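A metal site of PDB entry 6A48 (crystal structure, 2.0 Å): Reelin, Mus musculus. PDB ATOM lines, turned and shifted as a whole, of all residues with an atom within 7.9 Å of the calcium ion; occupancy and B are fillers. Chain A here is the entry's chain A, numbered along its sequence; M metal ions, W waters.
Water W2 lies within hydrogen-bond range of OE2 of Glu 665 (2.5 Å) and OG of Ser 550 (2.9 Å).
Within 4 Å of the calcium ion: Ser 521, Ser 550, Lys 552 and Asp 664.
The nearest printed residue that does not touch the calcium ion is Gly 551 (4.04 Å).
OD1 of Asp 664 sits close to N of Ala 549 (3.2 Å).
The backbone carbonyl oxygen of Gly 523 is in hydrogen-bond range of the side-chain amino group of Lys 552.
The side-chain hydroxyl (OG) of Ser 521 lies within hydrogen-bond range of the side-chain carboxylate (OE2) of Glu 665, at 2.9 Å.
O of Ser 550 is bound to the calcium ion (2.3 Å).
O of Lys 552 is bound to the calcium ion.
The calcium ion is bound by O of Ser 521, 2.4 Å away.
The calcium ion is bound by water W2, at 2.5 Å.
OD2 of Asp 664 binds the calcium ion (2.6 Å).
The calcium ion is bound by water W1 (2.6 Å).
The calcium ion is bound by the side-chain carboxylate (OD1) of Asp 664, at 2.6 Å.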
ATOM      1  N   GLU A 520       8.821  22.836 -24.890  1.00  0.00           N
ATOM      2  CA  GLU A 520       9.021  21.452 -25.286  1.00  0.00           C
ATOM      3  C   GLU A 520       8.164  21.141 -26.504  1.00  0.00           C
ATOM      4  O   GLU A 520       6.941  21.259 -26.435  1.00  0.00           O
ATOM      5  CB  GLU A 520       8.692  20.491 -24.147  1.00  0.00           C
ATOM      6  CG  GLU A 520       9.134  19.072 -24.416  1.00  0.00           C
ATOM      7  CD  GLU A 520      10.560  19.011 -24.943  1.00  0.00           C
ATOM      8  OE1 GLU A 520      11.481  19.462 -24.230  1.00  0.00           O
ATOM      9  OE2 GLU A 520      10.759  18.516 -26.072  1.00  0.00           O
ATOM     10  N   SER A 521       8.813  20.751 -27.603  1.00  0.00           N
ATOM     11  CA  SER A 521       8.134  20.295 -28.808  1.00  0.00           C
ATOM     12  C   SER A 521       8.140  18.783 -28.954  1.00  0.00           C
ATOM     13  O   SER A 521       7.514  18.258 -29.892  1.00  0.00           O
ATOM     14  CB  SER A 521       8.787  20.916 -30.056  1.00  0.00           C
ATOM     15  OG  SER A 521       8.731  22.331 -30.015  1.00  0.00           O
ATOM     16  N   PHE A 522       8.832  18.066 -28.061  1.00  0.00           N
ATOM     17  CA  PHE A 522       8.840  16.596 -28.015  1.00  0.00           C
ATOM     18  C   PHE A 522       9.473  16.001 -29.269  1.00  0.00           C
ATOM     19  O   PHE A 522       8.929  15.085 -29.901  1.00  0.00           O
ATOM     20  CB  PHE A 522       7.427  16.044 -27.777  1.00  0.00           C
ATOM     21  CG  PHE A 522       6.854  16.423 -26.439  1.00  0.00           C
ATOM     22  CD1 PHE A 522       7.297  15.798 -25.279  1.00  0.00           C
ATOM     23  CD2 PHE A 522       5.887  17.407 -26.328  1.00  0.00           C
ATOM     24  CE1 PHE A 522       6.785  16.141 -24.044  1.00  0.00           C
ATOM     25  CE2 PHE A 522       5.373  17.764 -25.090  1.00  0.00           C
ATOM     26  CZ  PHE A 522       5.814  17.123 -23.947  1.00  0.00           C
ATOM     27  N   GLY A 523      10.655  16.511 -29.625  1.00  0.00           N
ATOM     28  CA  GLY A 523      11.417  15.933 -30.712  1.00  0.00           C
ATOM     29  C   GLY A 523      12.143  14.646 -30.374  1.00  0.00           C
ATOM     30  O   GLY A 523      12.440  13.852 -31.270  1.00  0.00           O
ATOM     31  N   VAL A 541       6.648   9.093 -26.951  1.00  0.00           N
ATOM     32  CA  VAL A 541       6.751  10.188 -27.900  1.00  0.00           C
ATOM     33  C   VAL A 541       6.676   9.595 -29.301  1.00  0.00           C
ATOM     34  O   VAL A 541       7.564   8.842 -29.707  1.00  0.00           O
ATOM     35  CB  VAL A 541       8.045  10.999 -27.707  1.00  0.00           C
ATOM     36  CG1 VAL A 541       8.201  12.022 -28.809  1.00  0.00           C
ATOM     37  CG2 VAL A 541       8.051  11.666 -26.345  1.00  0.00           C
ATOM     38  N   SER A 542       5.623   9.915 -30.036  1.00  0.00           N
ATOM     39  CA  SER A 542       5.366   9.269 -31.324  1.00  0.00           C
ATOM     40  C   SER A 542       4.302  10.066 -32.081  1.00  0.00           C
ATOM     41  O   SER A 542       3.864  11.130 -31.639  1.00  0.00           O
ATOM     42  CB  SER A 542       4.923   7.823 -31.130  1.00  0.00           C
ATOM     43  OG  SER A 542       3.630   7.777 -30.557  1.00  0.00           O
ATOM     44  N   PHE A 543       3.897   9.536 -33.240  1.00  0.00           N
ATOM     45  CA  PHE A 543       2.799  10.076 -34.043  1.00  0.00           C
ATOM     46  C   PHE A 543       1.476   9.371 -33.766  1.00  0.00           C
ATOM     47  O   PHE A 543       0.549   9.462 -34.588  1.00  0.00           O
ATOM     48  CB  PHE A 543       3.127   9.966 -35.538  1.00  0.00           C
ATOM     49  CG  PHE A 543       4.319  10.786 -35.968  1.00  0.00           C
ATOM     50  CD1 PHE A 543       4.178  12.131 -36.264  1.00  0.00           C
ATOM     51  CD2 PHE A 543       5.568  10.210 -36.092  1.00  0.00           C
ATOM     52  CE1 PHE A 543       5.261  12.889 -36.672  1.00  0.00           C
ATOM     53  CE2 PHE A 543       6.662  10.951 -36.491  1.00  0.00           C
ATOM     54  CZ  PHE A 543       6.515  12.291 -36.791  1.00  0.00           C
ATOM     55  N   GLY A 546      -1.513  11.380 -34.336  1.00  0.00           N
ATOM     56  CA  GLY A 546      -1.333  12.340 -35.398  1.00  0.00           C
ATOM     57  C   GLY A 546      -0.489  13.526 -34.944  1.00  0.00           C
ATOM     58  O   GLY A 546       0.142  13.522 -33.895  1.00  0.00           O
ATOM     59  N   VAL A 547      -0.499  14.554 -35.786  1.00  0.00           N
ATOM     60  CA  VAL A 547       0.234  15.787 -35.504  1.00  0.00           C
ATOM     61  C   VAL A 547      -0.672  16.718 -34.710  1.00  0.00           C
ATOM     62  O   VAL A 547      -1.798  17.026 -35.130  1.00  0.00           O
ATOM     63  CB  VAL A 547       0.705  16.464 -36.810  1.00  0.00           C
ATOM     64  CG1 VAL A 547       1.384  17.785 -36.490  1.00  0.00           C
ATOM     65  CG2 VAL A 547       1.645  15.540 -37.568  1.00  0.00           C
ATOM     66  N   LEU A 548      -0.195  17.164 -33.548  1.00  0.00           N
ATOM     67  CA  LEU A 548      -0.920  18.129 -32.743  1.00  0.00           C
ATOM     68  C   LEU A 548      -0.482  19.543 -33.071  1.00  0.00           C
ATOM     69  O   LEU A 548      -1.275  20.362 -33.550  1.00  0.00           O
ATOM     70  CB  LEU A 548      -0.734  17.821 -31.251  1.00  0.00           C
ATOM     71  CG  LEU A 548      -1.750  16.879 -30.601  1.00  0.00           C
ATOM     72  CD1 LEU A 548      -1.727  15.501 -31.246  1.00  0.00           C
ATOM     73  CD2 LEU A 548      -1.498  16.777 -29.105  1.00  0.00           C
ATOM     74  N   ALA A 549       0.789  19.855 -32.818  1.00  0.00           N
ATOM     75  CA  ALA A 549       1.362  21.109 -33.283  1.00  0.00           C
ATOM     76  C   ALA A 549       2.237  20.834 -34.493  1.00  0.00           C
ATOM     77  O   ALA A 549       1.834  21.118 -35.629  1.00  0.00           O
ATOM     78  CB  ALA A 549       2.178  21.776 -32.161  1.00  0.00           C
ATOM     79  N   SER A 550       3.414  20.277 -34.279  1.00  0.00           N
ATOM     80  CA  SER A 550       4.294  19.870 -35.359  1.00  0.00           C
ATOM     81  C   SER A 550       5.052  18.631 -34.928  1.00  0.00           C
ATOM     82  O   SER A 550       5.400  18.478 -33.751  1.00  0.00           O
ATOM     83  CB  SER A 550       5.282  20.983 -35.736  1.00  0.00           C
ATOM     84  OG  SER A 550       6.200  21.231 -34.676  1.00  0.00           O
ATOM     85  N   GLY A 551       5.306  17.734 -35.884  1.00  0.00           N
ATOM     86  CA  GLY A 551       6.085  16.549 -35.593  1.00  0.00           C
ATOM     87  C   GLY A 551       5.382  15.629 -34.609  1.00  0.00           C
ATOM     88  O   GLY A 551       4.163  15.486 -34.609  1.00  0.00           O
ATOM     89  N   LYS A 552       6.182  15.000 -33.751  1.00  0.00           N
ATOM     90  CA  LYS A 552       5.665  14.060 -32.772  1.00  0.00           C
ATOM     91  C   LYS A 552       5.019  14.791 -31.595  1.00  0.00           C
ATOM     92  O   LYS A 552       5.182  15.998 -31.407  1.00  0.00           O
ATOM     93  CB  LYS A 552       6.777  13.130 -32.279  1.00  0.00           C
ATOM     94  CG  LYS A 552       7.396  12.263 -33.368  1.00  0.00           C
ATOM     95  CD  LYS A 552       8.441  11.318 -32.824  1.00  0.00           C
ATOM     96  CE  LYS A 552       9.621  12.068 -32.202  1.00  0.00           C
ATOM     97  NZ  LYS A 552      10.391  12.884 -33.192  1.00  0.00           N
ATOM     98  N   ALA A 553       4.276  14.023 -30.790  1.00  0.00           N
ATOM     99  CA  ALA A 553       3.660  14.521 -29.577  1.00  0.00           C
ATOM    100  C   ALA A 553       3.905  13.519 -28.456  1.00  0.00           C
ATOM    101  O   ALA A 553       4.427  12.422 -28.685  1.00  0.00           O
ATOM    102  CB  ALA A 553       2.148  14.773 -29.769  1.00  0.00           C
ATOM    103  N   LEU A 554       3.529  13.893 -27.235  1.00  0.00           N
ATOM    104  CA  LEU A 554       3.606  13.004 -26.092  1.00  0.00           C
ATOM    105  C   LEU A 554       2.262  12.294 -25.967  1.00  0.00           C
ATOM    106  O   LEU A 554       1.248  12.911 -25.637  1.00  0.00           O
ATOM    107  CB  LEU A 554       3.949  13.759 -24.817  1.00  0.00           C
ATOM    108  CG  LEU A 554       4.181  12.902 -23.572  1.00  0.00           C
ATOM    109  CD1 LEU A 554       5.335  11.917 -23.791  1.00  0.00           C
ATOM    110  CD2 LEU A 554       4.445  13.764 -22.350  1.00  0.00           C
ATOM    111  N   ILE A 663      -0.348  15.465 -25.835  1.00  0.00           N
ATOM    112  CA  ILE A 663       0.011  16.853 -25.556  1.00  0.00           C
ATOM    113  C   ILE A 663       1.254  17.204 -26.368  1.00  0.00           C
ATOM    114  O   ILE A 663       2.053  16.323 -26.702  1.00  0.00           O
ATOM    115  CB  ILE A 663       0.226  17.079 -24.043  1.00  0.00           C
ATOM    116  CG1 ILE A 663       0.210  18.559 -23.691  1.00  0.00           C
ATOM    117  CG2 ILE A 663       1.512  16.412 -23.581  1.00  0.00           C
ATOM    118  CD1 ILE A 663       0.099  18.816 -22.222  1.00  0.00           C
ATOM    119  N   ASP A 664       1.401  18.479 -26.689  1.00  0.00           N
ATOM    120  CA  ASP A 664       2.525  18.908 -27.521  1.00  0.00           C
ATOM    121  C   ASP A 664       2.690  20.414 -27.380  1.00  0.00           C
ATOM    122  O   ASP A 664       1.737  21.128 -27.030  1.00  0.00           O
ATOM    123  CB  ASP A 664       2.285  18.507 -28.982  1.00  0.00           C
ATOM    124  CG  ASP A 664       3.485  18.784 -29.877  1.00  0.00           C
ATOM    125  OD1 ASP A 664       3.292  18.811 -31.106  1.00  0.00           O
ATOM    126  OD2 ASP A 664       4.609  18.944 -29.359  1.00  0.00           O
ATOM    127  N   GLU A 665       3.909  20.888 -27.638  1.00  0.00           N
ATOM    128  CA  GLU A 665       4.198  22.313 -27.764  1.00  0.00           C
ATOM    129  C   GLU A 665       3.819  23.082 -26.493  1.00  0.00           C
ATOM    130  O   GLU A 665       2.972  23.977 -26.489  1.00  0.00           O
ATOM    131  CB  GLU A 665       3.488  22.900 -28.996  1.00  0.00           C
ATOM    132  CG  GLU A 665       4.146  24.132 -29.575  1.00  0.00           C
ATOM    133  CD  GLU A 665       5.564  23.868 -30.055  1.00  0.00           C
ATOM    134  OE1 GLU A 665       6.385  24.804 -30.005  1.00  0.00           O
ATOM    135  OE2 GLU A 665       5.852  22.729 -30.492  1.00  0.00           O
ATOM    136  N   ILE A 666       4.471  22.714 -25.401  1.00  0.00           N
ATOM    137  CA  ILE A 666       4.267  23.347 -24.103  1.00  0.00           C
ATOM    138  C   ILE A 666       5.180  24.559 -24.005  1.00  0.00           C
ATOM    139  O   ILE A 666       6.396  24.436 -24.199  1.00  0.00           O
ATOM    140  CB  ILE A 666       4.535  22.355 -22.960  1.00  0.00           C
ATOM    141  CG1 ILE A 666       3.655  21.122 -23.100  1.00  0.00           C
ATOM    142  CG2 ILE A 666       4.350  23.021 -21.601  1.00  0.00           C
ATOM    143  CD1 ILE A 666       4.050  19.992 -22.188  1.00  0.00           C
HETATM  144 CA    CA M   1       5.810  18.205 -31.529  1.00  0.00          CA
HETATM  145  O   HOH W   1       8.115  18.464 -32.736  1.00  0.00           O
HETATM  146  O   HOH W   2       5.664  20.654 -31.866  1.00  0.00           O
